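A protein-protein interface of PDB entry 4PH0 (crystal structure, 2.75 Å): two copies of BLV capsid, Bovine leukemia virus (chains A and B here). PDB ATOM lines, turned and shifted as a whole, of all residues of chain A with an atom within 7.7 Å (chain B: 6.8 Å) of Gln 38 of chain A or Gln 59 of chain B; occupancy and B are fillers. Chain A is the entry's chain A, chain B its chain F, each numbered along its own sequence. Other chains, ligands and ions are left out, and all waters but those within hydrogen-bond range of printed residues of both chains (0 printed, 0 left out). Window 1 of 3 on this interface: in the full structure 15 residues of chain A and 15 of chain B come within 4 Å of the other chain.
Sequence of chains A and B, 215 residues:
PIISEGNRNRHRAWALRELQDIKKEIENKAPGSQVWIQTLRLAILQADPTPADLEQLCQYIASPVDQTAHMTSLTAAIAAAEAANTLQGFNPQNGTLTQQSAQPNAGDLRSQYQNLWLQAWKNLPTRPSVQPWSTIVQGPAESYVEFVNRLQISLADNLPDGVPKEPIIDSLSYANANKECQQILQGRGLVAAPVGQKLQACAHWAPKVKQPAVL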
ATOM      1  N   ILE A  26      -3.754  23.773  22.301  1.00  0.00           N
ATOM      2  CA  ILE A  26      -3.419  22.748  23.265  1.00  0.00           C
ATOM      3  C   ILE A  26      -3.446  21.338  22.682  1.00  0.00           C
ATOM      4  O   ILE A  26      -2.917  20.415  23.293  1.00  0.00           O
ATOM      5  CB  ILE A  26      -4.378  22.810  24.451  1.00  0.00           C
ATOM      6  CG1 ILE A  26      -3.767  22.159  25.682  1.00  0.00           C
ATOM      7  CG2 ILE A  26      -5.678  22.154  24.101  1.00  0.00           C
ATOM      8  CD1 ILE A  26      -4.530  22.451  26.934  1.00  0.00           C
ATOM      9  N   GLY A  32      -1.411  18.030  32.049  1.00  0.00           N
ATOM     10  CA  GLY A  32      -0.595  18.357  33.200  1.00  0.00           C
ATOM     11  C   GLY A  32       0.824  18.768  32.845  1.00  0.00           C
ATOM     12  O   GLY A  32       1.597  19.120  33.739  1.00  0.00           O
ATOM     13  N   SER A  33       1.186  18.703  31.560  1.00  0.00           N
ATOM     14  CA  SER A  33       2.510  19.159  31.121  1.00  0.00           C
ATOM     15  C   SER A  33       2.538  20.673  31.282  1.00  0.00           C
ATOM     16  O   SER A  33       1.486  21.309  31.263  1.00  0.00           O
ATOM     17  CB  SER A  33       2.820  18.748  29.673  1.00  0.00           C
ATOM     18  OG  SER A  33       1.974  19.379  28.726  1.00  0.00           O
ATOM     19  N   GLN A  34       3.715  21.257  31.480  1.00  0.00           N
ATOM     20  CA  GLN A  34       3.758  22.679  31.781  1.00  0.00           C
ATOM     21  C   GLN A  34       3.144  23.489  30.640  1.00  0.00           C
ATOM     22  O   GLN A  34       2.349  24.397  30.872  1.00  0.00           O
ATOM     23  CB  GLN A  34       5.181  23.145  32.071  1.00  0.00           C
ATOM     24  CG  GLN A  34       5.255  24.601  32.570  1.00  0.00           C
ATOM     25  CD  GLN A  34       4.441  24.833  33.854  1.00  0.00           C
ATOM     26  OE1 GLN A  34       3.207  24.751  33.856  1.00  0.00           O
ATOM     27  NE2 GLN A  34       5.141  25.137  34.951  1.00  0.00           N
ATOM     28  N   VAL A  35       3.517  23.137  29.412  1.00  0.00           N
ATOM     29  CA  VAL A  35       3.014  23.801  28.212  1.00  0.00           C
ATOM     30  C   VAL A  35       1.500  23.690  28.178  1.00  0.00           C
ATOM     31  O   VAL A  35       0.804  24.634  27.816  1.00  0.00           O
ATOM     32  CB  VAL A  35       3.630  23.202  26.919  1.00  0.00           C
ATOM     33  CG1 VAL A  35       3.641  21.676  26.960  1.00  0.00           C
ATOM     34  CG2 VAL A  35       2.911  23.721  25.670  1.00  0.00           C
ATOM     35  N   TRP A  36       1.002  22.516  28.542  1.00  0.00           N
ATOM     36  CA  TRP A  36      -0.420  22.314  28.715  1.00  0.00           C
ATOM     37  C   TRP A  36      -0.959  23.339  29.689  1.00  0.00           C
ATOM     38  O   TRP A  36      -1.878  24.087  29.377  1.00  0.00           O
ATOM     39  CB  TRP A  36      -0.686  20.893  29.204  1.00  0.00           C
ATOM     40  CG  TRP A  36      -2.088  20.594  29.615  1.00  0.00           C
ATOM     41  CD1 TRP A  36      -2.677  20.930  30.794  1.00  0.00           C
ATOM     42  CD2 TRP A  36      -3.077  19.875  28.864  1.00  0.00           C
ATOM     43  NE1 TRP A  36      -3.972  20.482  30.824  1.00  0.00           N
ATOM     44  CE2 TRP A  36      -4.246  19.832  29.650  1.00  0.00           C
ATOM     45  CE3 TRP A  36      -3.090  19.271  27.604  1.00  0.00           C
ATOM     46  CZ2 TRP A  36      -5.418  19.210  29.215  1.00  0.00           C
ATOM     47  CZ3 TRP A  36      -4.260  18.652  27.174  1.00  0.00           C
ATOM     48  CH2 TRP A  36      -5.406  18.625  27.983  1.00  0.00           C
ATOM     49  N   ILE A  37      -0.379  23.363  30.877  1.00  0.00           N
ATOM     50  CA  ILE A  37      -0.852  24.240  31.936  1.00  0.00           C
ATOM     51  C   ILE A  37      -0.659  25.734  31.651  1.00  0.00           C
ATOM     52  O   ILE A  37      -1.535  26.543  31.926  1.00  0.00           O
ATOM     53  CB  ILE A  37      -0.189  23.852  33.271  1.00  0.00           C
ATOM     54  CG1 ILE A  37      -0.721  22.484  33.714  1.00  0.00           C
ATOM     55  CG2 ILE A  37      -0.485  24.872  34.340  1.00  0.00           C
ATOM     56  CD1 ILE A  37      -0.105  21.945  34.984  1.00  0.00           C
ATOM     57  N   GLN A  38       0.484  26.107  31.102  1.00  0.00           N
ATOM     58  CA  GLN A  38       0.738  27.512  30.826  1.00  0.00           C
ATOM     59  C   GLN A  38      -0.203  28.025  29.729  1.00  0.00           C
ATOM     60  O   GLN A  38      -0.654  29.169  29.772  1.00  0.00           O
ATOM     61  CB  GLN A  38       2.206  27.737  30.471  1.00  0.00           C
ATOM     62  CG  GLN A  38       3.191  27.388  31.591  1.00  0.00           C
ATOM     63  CD  GLN A  38       4.606  27.863  31.277  1.00  0.00           C
ATOM     64  OE1 GLN A  38       5.033  27.844  30.127  1.00  0.00           O
ATOM     65  NE2 GLN A  38       5.311  28.351  32.294  1.00  0.00           N
ATOM     66  N   THR A  39      -0.492  27.170  28.751  1.00  0.00           N
ATOM     67  CA  THR A  39      -1.370  27.526  27.643  1.00  0.00           C
ATOM     68  C   THR A  39      -2.685  28.035  28.200  1.00  0.00           C
ATOM     69  O   THR A  39      -3.228  29.039  27.752  1.00  0.00           O
ATOM     70  CB  THR A  39      -1.642  26.309  26.722  1.00  0.00           C
ATOM     71  OG1 THR A  39      -0.400  25.731  26.299  1.00  0.00           O
ATOM     72  CG2 THR A  39      -2.458  26.712  25.503  1.00  0.00           C
ATOM     73  N   LEU A  40      -3.177  27.354  29.219  1.00  0.00           N
ATOM     74  CA  LEU A  40      -4.465  27.704  29.785  1.00  0.00           C
ATOM     75  C   LEU A  40      -4.409  28.988  30.592  1.00  0.00           C
ATOM     76  O   LEU A  40      -5.312  29.820  30.520  1.00  0.00           O
ATOM     77  CB  LEU A  40      -4.974  26.566  30.665  1.00  0.00           C
ATOM     78  CG  LEU A  40      -5.075  25.223  29.936  1.00  0.00           C
ATOM     79  CD1 LEU A  40      -5.641  24.140  30.844  1.00  0.00           C
ATOM     80  CD2 LEU A  40      -5.868  25.337  28.636  1.00  0.00           C
ATOM     81  N   ARG A  41      -3.339  29.140  31.358  1.00  0.00           N
ATOM     82  CA  ARG A  41      -3.231  30.236  32.308  1.00  0.00           C
ATOM     83  C   ARG A  41      -3.403  31.584  31.623  1.00  0.00           C
ATOM     84  O   ARG A  41      -4.038  32.501  32.146  1.00  0.00           O
ATOM     85  CB  ARG A  41      -1.884  30.165  33.029  1.00  0.00           C
ATOM     86  CG  ARG A  41      -1.721  31.167  34.150  1.00  0.00           C
ATOM     87  CD  ARG A  41      -0.325  31.089  34.754  1.00  0.00           C
ATOM     88  NE  ARG A  41      -0.145  29.906  35.596  1.00  0.00           N
ATOM     89  CZ  ARG A  41      -0.533  29.810  36.865  1.00  0.00           C
ATOM     90  NH1 ARG A  41      -1.150  30.825  37.459  1.00  0.00           N
ATOM     91  NH2 ARG A  41      -0.322  28.687  37.540  1.00  0.00           N
ATOM     92  N   LEU A  42      -2.839  31.680  30.431  1.00  0.00           N
ATOM     93  CA  LEU A  42      -2.924  32.891  29.648  1.00  0.00           C
ATOM     94  C   LEU A  42      -4.355  33.083  29.188  1.00  0.00           C
ATOM     95  O   LEU A  42      -4.881  34.194  29.209  1.00  0.00           O
ATOM     96  CB  LEU A  42      -1.933  32.837  28.497  1.00  0.00           C
ATOM     97  CG  LEU A  42      -1.880  34.014  27.535  1.00  0.00           C
ATOM     98  CD1 LEU A  42      -1.798  35.344  28.263  1.00  0.00           C
ATOM     99  CD2 LEU A  42      -0.605  33.796  26.763  1.00  0.00           C
ATOM    100  N   ALA A  43      -4.964  31.996  28.736  1.00  0.00           N
ATOM    101  CA  ALA A  43      -6.336  32.039  28.289  1.00  0.00           C
ATOM    102  C   ALA A  43      -7.221  32.640  29.384  1.00  0.00           C
ATOM    103  O   ALA A  43      -8.097  33.448  29.101  1.00  0.00           O
ATOM    104  CB  ALA A  43      -6.810  30.664  27.909  1.00  0.00           C
ATOM    105  N   ILE A  44      -6.982  32.247  30.631  1.00  0.00           N
ATOM    106  CA  ILE A  44      -7.754  32.755  31.775  1.00  0.00           C
ATOM    107  C   ILE A  44      -7.708  34.269  31.864  1.00  0.00           C
ATOM    108  O   ILE A  44      -8.691  34.929  32.208  1.00  0.00           O
ATOM    109  CB  ILE A  44      -7.255  32.177  33.102  1.00  0.00           C
ATOM    110  CG1 ILE A  44      -7.764  30.755  33.261  1.00  0.00           C
ATOM    111  CG2 ILE A  44      -7.759  32.986  34.286  1.00  0.00           C
ATOM    112  CD1 ILE A  44      -7.176  30.046  34.437  1.00  0.00           C
ATOM    113  N   LEU A  45      -6.535  34.804  31.579  1.00  0.00           N
ATOM    114  CA  LEU A  45      -6.313  36.231  31.621  1.00  0.00           C
ATOM    115  C   LEU A  45      -7.205  36.923  30.612  1.00  0.00           C
ATOM    116  O   LEU A  45      -7.596  38.072  30.802  1.00  0.00           O
ATOM    117  CB  LEU A  45      -4.858  36.552  31.341  1.00  0.00           C
ATOM    118  CG  LEU A  45      -3.948  35.869  32.353  1.00  0.00           C
ATOM    119  CD1 LEU A  45      -2.492  36.074  31.982  1.00  0.00           C
ATOM    120  CD2 LEU A  45      -4.246  36.368  33.750  1.00  0.00           C
ATOM    121  N   LEU A 118      -6.163  25.273  37.832  1.00  0.00           N
ATOM    122  CA  LEU A 118      -4.993  24.952  37.053  1.00  0.00           C
ATOM    123  C   LEU A 118      -4.237  23.817  37.686  1.00  0.00           C
ATOM    124  O   LEU A 118      -3.924  22.824  37.044  1.00  0.00           O
ATOM    125  CB  LEU A 118      -4.092  26.175  36.956  1.00  0.00           C
ATOM    126  CG  LEU A 118      -4.629  27.303  36.086  1.00  0.00           C
ATOM    127  CD1 LEU A 118      -3.808  28.562  36.275  1.00  0.00           C
ATOM    128  CD2 LEU A 118      -4.599  26.873  34.642  1.00  0.00           C
ATOM    129  N   ALA A 156       9.548  21.310  35.900  1.00  0.00           N
ATOM    130  CA  ALA A 156       8.342  22.110  35.738  1.00  0.00           C
ATOM    131  C   ALA A 156       7.144  21.197  35.629  1.00  0.00           C
ATOM    132  O   ALA A 156       6.020  21.554  35.974  1.00  0.00           O
ATOM    133  CB  ALA A 156       8.458  22.995  34.512  1.00  0.00           C
ATOM    134  N   LEU B  54       6.316  39.913  28.126  1.00  0.00           N
ATOM    135  CA  LEU B  54       7.432  39.351  27.378  1.00  0.00           C
ATOM    136  C   LEU B  54       7.862  37.983  27.858  1.00  0.00           C
ATOM    137  O   LEU B  54       8.182  37.109  27.049  1.00  0.00           O
ATOM    138  CB  LEU B  54       8.610  40.305  27.437  1.00  0.00           C
ATOM    139  CG  LEU B  54       8.263  41.577  26.674  1.00  0.00           C
ATOM    140  CD1 LEU B  54       9.338  42.617  26.850  1.00  0.00           C
ATOM    141  CD2 LEU B  54       8.074  41.248  25.208  1.00  0.00           C
ATOM    142  N   GLU B  55       7.884  37.799  29.171  1.00  0.00           N
ATOM    143  CA  GLU B  55       8.220  36.501  29.723  1.00  0.00           C
ATOM    144  C   GLU B  55       7.192  35.512  29.192  1.00  0.00           C
ATOM    145  O   GLU B  55       7.519  34.372  28.873  1.00  0.00           O
ATOM    146  CB  GLU B  55       8.225  36.531  31.253  1.00  0.00           C
ATOM    147  CG  GLU B  55       9.256  37.475  31.865  1.00  0.00           C
ATOM    148  CD  GLU B  55       9.358  37.342  33.384  1.00  0.00           C
ATOM    149  OE1 GLU B  55       8.540  36.613  33.983  1.00  0.00           O
ATOM    150  OE2 GLU B  55      10.262  37.967  33.983  1.00  0.00           O
ATOM    151  N   GLN B  56       5.954  35.980  29.059  1.00  0.00           N
ATOM    152  CA  GLN B  56       4.865  35.160  28.536  1.00  0.00           C
ATOM    153  C   GLN B  56       5.197  34.675  27.129  1.00  0.00           C
ATOM    154  O   GLN B  56       4.916  33.539  26.761  1.00  0.00           O
ATOM    155  CB  GLN B  56       3.549  35.953  28.546  1.00  0.00           C
ATOM    156  CG  GLN B  56       3.067  36.351  29.949  1.00  0.00           C
ATOM    157  CD  GLN B  56       1.888  37.309  29.927  1.00  0.00           C
ATOM    158  OE1 GLN B  56       1.146  37.368  28.956  1.00  0.00           O
ATOM    159  NE2 GLN B  56       1.720  38.071  30.999  1.00  0.00           N
ATOM    160  N   LEU B  57       5.803  35.548  26.344  1.00  0.00           N
ATOM    161  CA  LEU B  57       6.192  35.209  24.987  1.00  0.00           C
ATOM    162  C   LEU B  57       7.206  34.089  24.882  1.00  0.00           C
ATOM    163  O   LEU B  57       7.048  33.205  24.044  1.00  0.00           O
ATOM    164  CB  LEU B  57       6.748  36.435  24.295  1.00  0.00           C
ATOM    165  CG  LEU B  57       5.650  37.478  24.156  1.00  0.00           C
ATOM    166  CD1 LEU B  57       6.190  38.723  23.491  1.00  0.00           C
ATOM    167  CD2 LEU B  57       4.462  36.906  23.391  1.00  0.00           C
ATOM    168  N   CYS B  58       8.234  34.137  25.735  1.00  0.00           N
ATOM    169  CA  CYS B  58       9.311  33.143  25.745  1.00  0.00           C
ATOM    170  C   CYS B  58       8.789  31.719  25.703  1.00  0.00           C
ATOM    171  O   CYS B  58       9.319  30.866  24.998  1.00  0.00           O
ATOM    172  CB  CYS B  58      10.168  33.279  27.004  1.00  0.00           C
ATOM    173  SG  CYS B  58      11.283  34.679  27.132  1.00  0.00           S
ATOM    174  N   GLN B  59       7.736  31.486  26.472  1.00  0.00           N
ATOM    175  CA  GLN B  59       7.190  30.156  26.695  1.00  0.00           C
ATOM    176  C   GLN B  59       6.378  29.582  25.525  1.00  0.00           C
ATOM    177  O   GLN B  59       6.370  28.369  25.310  1.00  0.00           O
ATOM    178  CB  GLN B  59       6.353  30.197  27.963  1.00  0.00           C
ATOM    179  CG  GLN B  59       7.164  30.730  29.142  1.00  0.00           C
ATOM    180  CD  GLN B  59       6.318  30.961  30.373  1.00  0.00           C
ATOM    181  OE1 GLN B  59       5.102  30.743  30.366  1.00  0.00           O
ATOM    182  NE2 GLN B  59       6.943  31.485  31.421  1.00  0.00           N
ATOM    183  N   TYR B  60       5.719  30.449  24.761  1.00  0.00           N
ATOM    184  CA  TYR B  60       4.869  29.999  23.655  1.00  0.00           C
ATOM    185  C   TYR B  60       5.717  29.548  22.491  1.00  0.00           C
ATOM    186  O   TYR B  60       5.366  28.634  21.742  1.00  0.00           O
ATOM    187  CB  TYR B  60       3.939  31.129  23.198  1.00  0.00           C
ATOM    188  CG  TYR B  60       2.828  30.738  22.237  1.00  0.00           C
ATOM    189  CD1 TYR B  60       1.571  30.357  22.684  1.00  0.00           C
ATOM    190  CD2 TYR B  60       3.035  30.794  20.867  1.00  0.00           C
ATOM    191  CE1 TYR B  60       0.566  30.027  21.786  1.00  0.00           C
ATOM    192  CE2 TYR B  60       2.044  30.467  19.978  1.00  0.00           C
ATOM    193  CZ  TYR B  60       0.816  30.084  20.432  1.00  0.00           C
ATOM    194  OH  TYR B  60      -0.156  29.764  19.510  1.00  0.00           O
ATOM    195  N   ILE B  61       6.845  30.221  22.350  1.00  0.00           N
ATOM    196  CA  ILE B  61       7.679  30.067  21.187  1.00  0.00           C
ATOM    197  C   ILE B  61       8.984  29.313  21.410  1.00  0.00           C
ATOM    198  O   ILE B  61       9.518  28.736  20.462  1.00  0.00           O
ATOM    199  CB  ILE B  61       7.991  31.431  20.631  1.00  0.00           C
ATOM    200  CG1 ILE B  61       8.694  32.262  21.698  1.00  0.00           C
ATOM    201  CG2 ILE B  61       6.701  32.120  20.279  1.00  0.00           C
ATOM    202  CD1 ILE B  61       9.177  33.603  21.218  1.00  0.00           C
ATOM    203  N   ALA B  62       9.500  29.309  22.642  1.00  0.00           N
ATOM    204  CA  ALA B  62      10.852  28.807  22.862  1.00  0.00           C
ATOM    205  C   ALA B  62      10.943  27.594  23.761  1.00  0.00           C
ATOM    206  O   ALA B  62      10.200  27.461  24.725  1.00  0.00           O
ATOM    207  CB  ALA B  62      11.718  29.909  23.425  1.00  0.00           C
ATOM    208  N   SER B  63      11.898  26.726  23.451  1.00  0.00           N
ATOM    209  CA  SER B  63      12.196  25.619  24.325  1.00  0.00           C
ATOM    210  C   SER B  63      12.754  26.223  25.592  1.00  0.00           C
ATOM    211  O   SER B  63      13.395  27.272  25.551  1.00  0.00           O
ATOM    212  CB  SER B  63      13.201  24.650  23.698  1.00  0.00           C
ATOM    213  OG  SER B  63      14.452  25.275  23.477  1.00  0.00           O
ATOM    214  N   GLN B  67      14.727  29.584  26.586  1.00  0.00           N
ATOM    215  CA  GLN B  67      14.110  30.529  27.506  1.00  0.00           C
ATOM    216  C   GLN B  67      15.121  30.986  28.534  1.00  0.00           C
ATOM    217  O   GLN B  67      15.180  32.157  28.900  1.00  0.00           O
ATOM    218  CB  GLN B  67      12.924  29.893  28.200  1.00  0.00           C
ATOM    219  CG  GLN B  67      11.885  29.433  27.239  1.00  0.00           C
ATOM    220  CD  GLN B  67      10.768  28.734  27.938  1.00  0.00           C
ATOM    221  OE1 GLN B  67      10.466  29.026  29.097  1.00  0.00           O
ATOM    222  NE2 GLN B  67      10.159  27.775  27.254  1.00  0.00           N
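The side-chain amide oxygen (OE1) of Gln 38 of chain A lies close to the side-chain amide oxygen (OE1) of Gln 59 of chain B (2.9 Å).
Leu 42 of chain A touches Gln 56 of chain B (CD1 to OE1, 3.6 Å).
Gln 38 of chain A touches just one residue of chain B: Gln 59.
Gln 59 of chain B touches just one residue of chain A: Gln 38.
Printed residues of chain A within 4 Å of Gln 56 of chain B: Leu 42 (3.6 Å).
Printed residues of chain B within 4 Å of Leu 42 of chain A: Gln 56 (3.6 Å).
Tyr 60 of chain B touches none of the printed residues of chain A.
The nearest residue of chain B that does not touch Gln 38 of chain A is Gln 67 of chain B (5.7 Å).
The nearest residue of chain A that does not touch Gln 59 of chain B is Val 35 of chain A (5.8 Å).
The nearest printed residue of chain B that does not touch Leu 42 of chain A is Tyr 60 of chain B (5.8 Å).
Printed residues of chain A that touch a printed residue of chain B: Gln 38 and Leu 42.
Hydrophobic or aromatic side chains of chain A within 4 Å of the printed part of chain B: Leu 42.
Along chain A the printed residues that touch a printed residue of chain B span positions 38 to 42.
Among the printed residues, no Asp or Glu carboxylate lies within 4 Å of a Lys or Arg side-chain nitrogen of the other chain.
No position is printed for both chains.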
